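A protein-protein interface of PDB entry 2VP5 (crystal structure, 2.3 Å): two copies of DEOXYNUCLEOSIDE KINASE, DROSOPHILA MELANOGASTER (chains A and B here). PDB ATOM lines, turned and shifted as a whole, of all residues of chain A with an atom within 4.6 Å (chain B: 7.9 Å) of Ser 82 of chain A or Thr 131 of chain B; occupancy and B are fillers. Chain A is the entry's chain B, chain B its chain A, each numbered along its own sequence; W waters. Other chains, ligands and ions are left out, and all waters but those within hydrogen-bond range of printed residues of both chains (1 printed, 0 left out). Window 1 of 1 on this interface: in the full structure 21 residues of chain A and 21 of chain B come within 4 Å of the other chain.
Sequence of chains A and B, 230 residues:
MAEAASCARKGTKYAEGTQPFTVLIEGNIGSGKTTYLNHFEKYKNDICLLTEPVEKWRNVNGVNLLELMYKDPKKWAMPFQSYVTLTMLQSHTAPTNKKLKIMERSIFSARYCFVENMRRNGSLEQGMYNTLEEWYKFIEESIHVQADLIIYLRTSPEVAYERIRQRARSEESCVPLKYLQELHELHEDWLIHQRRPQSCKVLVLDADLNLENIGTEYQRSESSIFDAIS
NE1 of Trp 135 of chain B sits at hydrogen-bond distance from OG of Ser 82 of chain A.
O of Gly 127 of chain B sits at hydrogen-bond distance from OG1 of Thr 131 of chain B (3.0 Å).
Gly 127 of chain B touches Leu 65 of chain A (O to CD2, 3.9 Å). Leu 65 of chain A touches Thr 131 of chain B (CD1 to OG1, 3.3 Å). Pro 79 of chain B touches Met 78 of chain A. Met 128 of chain B touches Pro 79 of chain A (CG to CG, 3.9 Å). Thr 131 of chain B touches Pro 79 of chain A (CG2 to O, 3.7 Å). OG of Ser 82 of chain A touches CG2 of Thr 131 of chain B (3.95 Å). Tyr 83 of chain A touches Thr 131 of chain B. CE1 of Tyr 83 of chain A touches CG of Glu 134 of chain B (3.5 Å). Leu 86 of chain A touches Glu 134 of chain B (CD2 to C, 3.5 Å). Leu 86 of chain A touches Trp 135 of chain B (CD2 to N, 3.5 Å).
Printed residues of chain B within 4 Å of Tyr 83 of chain A: Thr 131 (3.97 Å) and Glu 134 (3.5 Å). Of the printed residues of chain A, Trp 135 of chain B touches Ser 82 and Leu 86. Of the printed residues of chain A, Glu 134 of chain B touches Tyr 83 and Leu 86. Gln 81 of chain A touches none of the printed residues of chain B. Leu 132 of chain A touches none of the printed residues of chain B. The nearest residue of chain B that does not touch Ser 82 of chain A is Ser 82 of chain B (4.4 Å). The nearest printed residue of chain B that does not touch Leu 65 of chain A is Met 128 of chain B (5.1 Å).
Of the 16 printed residues of chain B, 6 touch a printed residue of chain A. Hydrophobic or aromatic side chains of chain B that line the printed part of chain A: Pro 79, Met 128 and Trp 135. Of the 11 printed residues of chain A, 6 touch a printed residue of chain B. Printed residues of chain A that touch a printed residue of chain B: Leu 65, Met 78, Pro 79, Ser 82, Tyr 83 and Leu 86. Hydrophobic or aromatic side chains of chain A within 4 Å of the printed part of chain B: Leu 65, Met 78, Pro 79, Tyr 83 and Leu 86. Among the printed residues, 11 pairs touch across the chains.
Met 78 of chain A touches Pro 79 of chain B, but with the chains exchanged Pro 79 of chain A does not touch Met 78 of chain B (4.003 Å).
Water W1 bridges the side-chain hydroxyl (OG) of Ser 82 of chain A (2.5 Å) and the side-chain hydroxyl (OG) of Ser 82 of chain B (2.8 Å).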
ATOM      1  N   LEU A  65      13.182  19.888   4.568  1.00  0.00           N
ATOM      2  CA  LEU A  65      13.849  19.020   5.543  1.00  0.00           C
ATOM      3  C   LEU A  65      13.290  17.604   5.522  1.00  0.00           C
ATOM      4  O   LEU A  65      14.030  16.641   5.766  1.00  0.00           O
ATOM      5  CB  LEU A  65      13.732  19.598   6.958  1.00  0.00           C
ATOM      6  CG  LEU A  65      14.628  20.775   7.360  1.00  0.00           C
ATOM      7  CD1 LEU A  65      14.339  21.112   8.800  1.00  0.00           C
ATOM      8  CD2 LEU A  65      16.105  20.468   7.159  1.00  0.00           C
ATOM      9  N   MET A  78      18.381  14.374  12.564  1.00  0.00           N
ATOM     10  CA  MET A  78      18.573  15.285  13.698  1.00  0.00           C
ATOM     11  C   MET A  78      17.927  16.663  13.491  1.00  0.00           C
ATOM     12  O   MET A  78      17.013  17.022  14.240  1.00  0.00           O
ATOM     13  CB  MET A  78      20.064  15.381  14.079  1.00  0.00           C
ATOM     14  CG  MET A  78      20.438  16.514  15.032  1.00  0.00           C
ATOM     15  SD  MET A  78      19.727  16.289  16.626  1.00  0.00           S
ATOM     16  CE  MET A  78      19.820  17.869  17.460  1.00  0.00           C
ATOM     17  N   PRO A  79      18.379  17.432  12.478  1.00  0.00           N
ATOM     18  CA  PRO A  79      17.712  18.722  12.253  1.00  0.00           C
ATOM     19  C   PRO A  79      16.199  18.592  11.956  1.00  0.00           C
ATOM     20  O   PRO A  79      15.383  19.351  12.505  1.00  0.00           O
ATOM     21  CB  PRO A  79      18.476  19.332  11.060  1.00  0.00           C
ATOM     22  CG  PRO A  79      19.269  18.231  10.454  1.00  0.00           C
ATOM     23  CD  PRO A  79      19.483  17.197  11.523  1.00  0.00           C
ATOM     24  N   PHE A  80      15.818  17.629  11.128  1.00  0.00           N
ATOM     25  CA  PHE A  80      14.396  17.388  10.875  1.00  0.00           C
ATOM     26  C   PHE A  80      13.553  17.206  12.150  1.00  0.00           C
ATOM     27  O   PHE A  80      12.575  17.929  12.358  1.00  0.00           O
ATOM     28  CB  PHE A  80      14.192  16.205   9.922  1.00  0.00           C
ATOM     29  CG  PHE A  80      12.746  15.885   9.672  1.00  0.00           C
ATOM     30  CD1 PHE A  80      11.958  16.734   8.908  1.00  0.00           C
ATOM     31  CD2 PHE A  80      12.161  14.751  10.234  1.00  0.00           C
ATOM     32  CE1 PHE A  80      10.613  16.447   8.695  1.00  0.00           C
ATOM     33  CE2 PHE A  80      10.829  14.461  10.027  1.00  0.00           C
ATOM     34  CZ  PHE A  80      10.055  15.309   9.249  1.00  0.00           C
ATOM     35  N   GLN A  81      13.930  16.252  13.005  1.00  0.00           N
ATOM     36  CA  GLN A  81      13.172  16.007  14.249  1.00  0.00           C
ATOM     37  C   GLN A  81      13.185  17.196  15.189  1.00  0.00           C
ATOM     38  O   GLN A  81      12.182  17.472  15.865  1.00  0.00           O
ATOM     39  CB  GLN A  81      13.653  14.749  14.982  1.00  0.00           C
ATOM     40  CG  GLN A  81      13.316  13.428  14.264  1.00  0.00           C
ATOM     41  CD  GLN A  81      11.814  13.217  13.999  1.00  0.00           C
ATOM     42  OE1 GLN A  81      10.961  13.696  14.734  1.00  0.00           O
ATOM     43  NE2 GLN A  81      11.504  12.482  12.947  1.00  0.00           N
ATOM     44  N   SER A  82      14.308  17.913  15.226  1.00  0.00           N
ATOM     45  CA  SER A  82      14.395  19.157  15.991  1.00  0.00           C
ATOM     46  C   SER A  82      13.365  20.184  15.515  1.00  0.00           C
ATOM     47  O   SER A  82      12.674  20.819  16.330  1.00  0.00           O
ATOM     48  CB  SER A  82      15.813  19.740  15.915  1.00  0.00           C
ATOM     49  OG  SER A  82      15.875  20.919  16.690  1.00  0.00           O
ATOM     50  N   TYR A  83      13.259  20.344  14.199  1.00  0.00           N
ATOM     51  CA  TYR A  83      12.245  21.228  13.612  1.00  0.00           C
ATOM     52  C   TYR A  83      10.811  20.702  13.784  1.00  0.00           C
ATOM     53  O   TYR A  83       9.869  21.476  13.973  1.00  0.00           O
ATOM     54  CB  TYR A  83      12.544  21.518  12.132  1.00  0.00           C
ATOM     55  CG  TYR A  83      11.694  22.641  11.593  1.00  0.00           C
ATOM     56  CD1 TYR A  83      11.745  23.912  12.165  1.00  0.00           C
ATOM     57  CD2 TYR A  83      10.824  22.430  10.521  1.00  0.00           C
ATOM     58  CE1 TYR A  83      10.959  24.942  11.687  1.00  0.00           C
ATOM     59  CE2 TYR A  83      10.033  23.452  10.036  1.00  0.00           C
ATOM     60  CZ  TYR A  83      10.105  24.707  10.621  1.00  0.00           C
ATOM     61  OH  TYR A  83       9.315  25.722  10.139  1.00  0.00           O
ATOM     62  N   VAL A  84      10.640  19.386  13.733  1.00  0.00           N
ATOM     63  CA  VAL A  84       9.354  18.797  14.093  1.00  0.00           C
ATOM     64  C   VAL A  84       8.970  19.209  15.516  1.00  0.00           C
ATOM     65  O   VAL A  84       7.875  19.738  15.717  1.00  0.00           O
ATOM     66  CB  VAL A  84       9.335  17.254  13.930  1.00  0.00           C
ATOM     67  CG1 VAL A  84       8.047  16.682  14.485  1.00  0.00           C
ATOM     68  CG2 VAL A  84       9.464  16.871  12.459  1.00  0.00           C
ATOM     69  N   THR A  85       9.864  18.987  16.485  1.00  0.00           N
ATOM     70  CA  THR A  85       9.617  19.354  17.892  1.00  0.00           C
ATOM     71  C   THR A  85       9.161  20.808  18.002  1.00  0.00           C
ATOM     72  O   THR A  85       8.207  21.123  18.714  1.00  0.00           O
ATOM     73  CB  THR A  85      10.890  19.182  18.753  1.00  0.00           C
ATOM     74  OG1 THR A  85      11.320  17.814  18.727  1.00  0.00           O
ATOM     75  CG2 THR A  85      10.639  19.602  20.190  1.00  0.00           C
ATOM     76  N   LEU A  86       9.845  21.689  17.277  1.00  0.00           N
ATOM     77  CA  LEU A  86       9.548  23.106  17.325  1.00  0.00           C
ATOM     78  C   LEU A  86       8.151  23.381  16.806  1.00  0.00           C
ATOM     79  O   LEU A  86       7.344  23.991  17.513  1.00  0.00           O
ATOM     80  CB  LEU A  86      10.592  23.916  16.543  1.00  0.00           C
ATOM     81  CG  LEU A  86      10.370  25.424  16.452  1.00  0.00           C
ATOM     82  CD1 LEU A  86      10.163  26.039  17.824  1.00  0.00           C
ATOM     83  CD2 LEU A  86      11.558  26.050  15.764  1.00  0.00           C
ATOM     84  N   LEU A 132      18.181  15.845  21.352  1.00  0.00           N
ATOM     85  CA  LEU A 132      16.725  15.837  21.192  1.00  0.00           C
ATOM     86  C   LEU A 132      15.998  15.538  22.510  1.00  0.00           C
ATOM     87  O   LEU A 132      15.008  16.196  22.833  1.00  0.00           O
ATOM     88  CB  LEU A 132      16.305  14.847  20.090  1.00  0.00           C
ATOM     89  CG  LEU A 132      16.708  15.227  18.656  1.00  0.00           C
ATOM     90  CD1 LEU A 132      16.441  14.114  17.694  1.00  0.00           C
ATOM     91  CD2 LEU A 132      16.017  16.492  18.180  1.00  0.00           C
ATOM     92  N   MET B  78      25.657  21.072  14.400  1.00  0.00           N
ATOM     93  CA  MET B  78      24.207  21.225  14.544  1.00  0.00           C
ATOM     94  C   MET B  78      23.692  20.773  15.916  1.00  0.00           C
ATOM     95  O   MET B  78      23.114  21.583  16.619  1.00  0.00           O
ATOM     96  CB  MET B  78      23.445  20.531  13.406  1.00  0.00           C
ATOM     97  CG  MET B  78      22.081  21.126  13.099  1.00  0.00           C
ATOM     98  SD  MET B  78      20.863  20.810  14.319  1.00  0.00           S
ATOM     99  CE  MET B  78      19.482  21.870  13.988  1.00  0.00           C
ATOM    100  N   PRO B  79      23.887  19.490  16.295  1.00  0.00           N
ATOM    101  CA  PRO B  79      23.433  19.097  17.640  1.00  0.00           C
ATOM    102  C   PRO B  79      24.124  19.859  18.780  1.00  0.00           C
ATOM    103  O   PRO B  79      23.453  20.272  19.740  1.00  0.00           O
ATOM    104  CB  PRO B  79      23.731  17.586  17.703  1.00  0.00           C
ATOM    105  CG  PRO B  79      24.662  17.309  16.597  1.00  0.00           C
ATOM    106  CD  PRO B  79      24.470  18.355  15.555  1.00  0.00           C
ATOM    107  N   SER B  82      22.603  23.346  19.043  1.00  0.00           N
ATOM    108  CA  SER B  82      21.255  23.183  19.556  1.00  0.00           C
ATOM    109  C   SER B  82      21.289  22.949  21.071  1.00  0.00           C
ATOM    110  O   SER B  82      20.472  23.488  21.817  1.00  0.00           O
ATOM    111  CB  SER B  82      20.546  22.028  18.846  1.00  0.00           C
ATOM    112  OG  SER B  82      19.260  21.842  19.412  1.00  0.00           O
ATOM    113  N   GLU B 125      25.195  23.303   7.116  1.00  0.00           N
ATOM    114  CA  GLU B 125      24.478  23.479   5.866  1.00  0.00           C
ATOM    115  C   GLU B 125      23.270  24.368   6.072  1.00  0.00           C
ATOM    116  O   GLU B 125      22.842  24.598   7.199  1.00  0.00           O
ATOM    117  CB  GLU B 125      24.080  22.132   5.284  1.00  0.00           C
ATOM    118  CG  GLU B 125      25.275  21.307   4.864  1.00  0.00           C
ATOM    119  CD  GLU B 125      24.909  20.145   3.992  1.00  0.00           C
ATOM    120  OE1 GLU B 125      25.629  19.128   4.048  1.00  0.00           O
ATOM    121  OE2 GLU B 125      23.913  20.243   3.242  1.00  0.00           O
ATOM    122  N   GLN B 126      22.731  24.879   4.972  1.00  0.00           N
ATOM    123  CA  GLN B 126      21.612  25.829   4.995  1.00  0.00           C
ATOM    124  C   GLN B 126      20.451  25.359   5.865  1.00  0.00           C
ATOM    125  O   GLN B 126      19.946  26.119   6.707  1.00  0.00           O
ATOM    126  CB  GLN B 126      21.142  26.118   3.559  1.00  0.00           C
ATOM    127  CG  GLN B 126      20.202  27.316   3.401  1.00  0.00           C
ATOM    128  CD  GLN B 126      20.844  28.626   3.847  1.00  0.00           C
ATOM    129  OE1 GLN B 126      21.923  28.996   3.375  1.00  0.00           O
ATOM    130  NE2 GLN B 126      20.179  29.334   4.768  1.00  0.00           N
ATOM    131  N   GLY B 127      20.042  24.106   5.674  1.00  0.00           N
ATOM    132  CA  GLY B 127      18.857  23.554   6.349  1.00  0.00           C
ATOM    133  C   GLY B 127      19.038  23.394   7.845  1.00  0.00           C
ATOM    134  O   GLY B 127      18.083  23.531   8.610  1.00  0.00           O
ATOM    135  N   MET B 128      20.271  23.105   8.253  1.00  0.00           N
ATOM    136  CA  MET B 128      20.646  22.998   9.662  1.00  0.00           C
ATOM    137  C   MET B 128      20.700  24.370  10.314  1.00  0.00           C
ATOM    138  O   MET B 128      20.161  24.569  11.405  1.00  0.00           O
ATOM    139  CB  MET B 128      21.995  22.309   9.793  1.00  0.00           C
ATOM    140  CG  MET B 128      21.962  20.852   9.458  1.00  0.00           C
ATOM    141  SD  MET B 128      23.631  20.346   9.103  1.00  0.00           S
ATOM    142  CE  MET B 128      23.340  18.787   8.268  1.00  0.00           C
ATOM    143  N   TYR B 129      21.345  25.316   9.636  1.00  0.00           N
ATOM    144  CA  TYR B 129      21.351  26.713  10.072  1.00  0.00           C
ATOM    145  C   TYR B 129      19.931  27.241  10.214  1.00  0.00           C
ATOM    146  O   TYR B 129      19.596  27.860  11.228  1.00  0.00           O
ATOM    147  CB  TYR B 129      22.165  27.567   9.093  1.00  0.00           C
ATOM    148  CG  TYR B 129      22.019  29.070   9.257  1.00  0.00           C
ATOM    149  CD1 TYR B 129      22.662  29.754  10.289  1.00  0.00           C
ATOM    150  CD2 TYR B 129      21.259  29.814   8.351  1.00  0.00           C
ATOM    151  CE1 TYR B 129      22.544  31.125  10.421  1.00  0.00           C
ATOM    152  CE2 TYR B 129      21.134  31.199   8.474  1.00  0.00           C
ATOM    153  CZ  TYR B 129      21.782  31.842   9.505  1.00  0.00           C
ATOM    154  OH  TYR B 129      21.652  33.210   9.622  1.00  0.00           O
ATOM    155  N   ASN B 130      19.103  27.001   9.195  1.00  0.00           N
ATOM    156  CA  ASN B 130      17.699  27.432   9.203  1.00  0.00           C
ATOM    157  C   ASN B 130      16.914  26.857  10.388  1.00  0.00           C
ATOM    158  O   ASN B 130      16.112  27.554  11.001  1.00  0.00           O
ATOM    159  CB  ASN B 130      17.009  27.066   7.876  1.00  0.00           C
ATOM    160  CG  ASN B 130      17.486  27.918   6.694  1.00  0.00           C
ATOM    161  OD1 ASN B 130      18.249  28.882   6.848  1.00  0.00           O
ATOM    162  ND2 ASN B 130      17.022  27.563   5.503  1.00  0.00           N
ATOM    163  N   THR B 131      17.157  25.597  10.722  1.00  0.00           N
ATOM    164  CA  THR B 131      16.499  24.976  11.892  1.00  0.00           C
ATOM    165  C   THR B 131      16.883  25.689  13.181  1.00  0.00           C
ATOM    166  O   THR B 131      16.008  26.041  13.969  1.00  0.00           O
ATOM    167  CB  THR B 131      16.797  23.465  11.996  1.00  0.00           C
ATOM    168  OG1 THR B 131      16.245  22.806  10.863  1.00  0.00           O
ATOM    169  CG2 THR B 131      16.189  22.855  13.258  1.00  0.00           C
ATOM    170  N   LEU B 132      18.182  25.913  13.376  1.00  0.00           N
ATOM    171  CA  LEU B 132      18.686  26.663  14.534  1.00  0.00           C
ATOM    172  C   LEU B 132      18.078  28.058  14.614  1.00  0.00           C
ATOM    173  O   LEU B 132      17.734  28.534  15.703  1.00  0.00           O
ATOM    174  CB  LEU B 132      20.224  26.744  14.505  1.00  0.00           C
ATOM    175  CG  LEU B 132      20.973  25.422  14.733  1.00  0.00           C
ATOM    176  CD1 LEU B 132      22.472  25.547  14.462  1.00  0.00           C
ATOM    177  CD2 LEU B 132      20.720  24.896  16.154  1.00  0.00           C
ATOM    178  N   GLU B 133      17.928  28.697  13.454  1.00  0.00           N
ATOM    179  CA  GLU B 133      17.366  30.046  13.362  1.00  0.00           C
ATOM    180  C   GLU B 133      15.891  30.104  13.696  1.00  0.00           C
ATOM    181  O   GLU B 133      15.432  31.086  14.273  1.00  0.00           O
ATOM    182  CB  GLU B 133      17.618  30.643  11.977  1.00  0.00           C
ATOM    183  CG  GLU B 133      18.959  31.338  11.855  1.00  0.00           C
ATOM    184  CD  GLU B 133      19.014  32.606  12.684  1.00  0.00           C
ATOM    185  OE1 GLU B 133      18.159  33.510  12.476  1.00  0.00           O
ATOM    186  OE2 GLU B 133      19.900  32.696  13.560  1.00  0.00           O
ATOM    187  N   GLU B 134      15.143  29.052  13.345  1.00  0.00           N
ATOM    188  CA  GLU B 134      13.722  28.965  13.707  1.00  0.00           C
ATOM    189  C   GLU B 134      13.539  28.845  15.207  1.00  0.00           C
ATOM    190  O   GLU B 134      12.610  29.431  15.770  1.00  0.00           O
ATOM    191  CB  GLU B 134      13.022  27.794  13.005  1.00  0.00           C
ATOM    192  CG  GLU B 134      12.796  27.961  11.508  1.00  0.00           C
ATOM    193  CD  GLU B 134      12.072  29.250  11.146  1.00  0.00           C
ATOM    194  OE1 GLU B 134      12.622  30.003  10.322  1.00  0.00           O
ATOM    195  OE2 GLU B 134      10.976  29.526  11.684  1.00  0.00           O
ATOM    196  N   TRP B 135      14.412  28.078  15.857  1.00  0.00           N
ATOM    197  CA  TRP B 135      14.411  28.010  17.319  1.00  0.00           C
ATOM    198  C   TRP B 135      14.659  29.385  17.970  1.00  0.00           C
ATOM    199  O   TRP B 135      13.923  29.783  18.875  1.00  0.00           O
ATOM    200  CB  TRP B 135      15.409  26.968  17.815  1.00  0.00           C
ATOM    201  CG  TRP B 135      14.819  25.585  17.917  1.00  0.00           C
ATOM    202  CD1 TRP B 135      15.042  24.529  17.071  1.00  0.00           C
ATOM    203  CD2 TRP B 135      13.901  25.110  18.917  1.00  0.00           C
ATOM    204  NE1 TRP B 135      14.330  23.437  17.488  1.00  0.00           N
ATOM    205  CE2 TRP B 135      13.625  23.760  18.620  1.00  0.00           C
ATOM    206  CE3 TRP B 135      13.297  25.693  20.043  1.00  0.00           C
ATOM    207  CZ2 TRP B 135      12.753  22.979  19.401  1.00  0.00           C
ATOM    208  CZ3 TRP B 135      12.434  24.915  20.830  1.00  0.00           C
ATOM    209  CH2 TRP B 135      12.169  23.571  20.500  1.00  0.00           C
ATOM    210  N   TYR B 136      15.666  30.114  17.477  1.00  0.00           N
ATOM    211  CA  TYR B 136      15.991  31.447  17.998  1.00  0.00           C
ATOM    212  C   TYR B 136      14.816  32.395  17.882  1.00  0.00           C
ATOM    213  O   TYR B 136      14.500  33.107  18.839  1.00  0.00           O
ATOM    214  CB  TYR B 136      17.210  32.059  17.296  1.00  0.00           C
ATOM    215  CG  TYR B 136      18.520  31.375  17.588  1.00  0.00           C
ATOM    216  CD1 TYR B 136      19.357  30.986  16.550  1.00  0.00           C
ATOM    217  CD2 TYR B 136      18.928  31.120  18.894  1.00  0.00           C
ATOM    218  CE1 TYR B 136      20.561  30.358  16.802  1.00  0.00           C
ATOM    219  CE2 TYR B 136      20.136  30.500  19.157  1.00  0.00           C
ATOM    220  CZ  TYR B 136      20.945  30.117  18.109  1.00  0.00           C
ATOM    221  OH  TYR B 136      22.150  29.491  18.345  1.00  0.00           O
ATOM    222  N   LYS B 137      14.174  32.395  16.714  1.00  0.00           N
ATOM    223  CA  LYS B 137      12.976  33.205  16.481  1.00  0.00           C
ATOM    224  C   LYS B 137      11.865  32.895  17.469  1.00  0.00           C
ATOM    225  O   LYS B 137      11.263  33.807  18.044  1.00  0.00           O
ATOM    226  CB  LYS B 137      12.445  32.988  15.074  1.00  0.00           C
ATOM    227  CG  LYS B 137      13.328  33.549  14.007  1.00  0.00           C
ATOM    228  CD  LYS B 137      12.568  33.652  12.709  1.00  0.00           C
ATOM    229  CE  LYS B 137      13.445  34.267  11.653  1.00  0.00           C
ATOM    230  NZ  LYS B 137      14.748  33.533  11.561  1.00  0.00           N
HETATM  231  O   HOH W   1      17.194  20.115  18.692  1.00  0.00           O
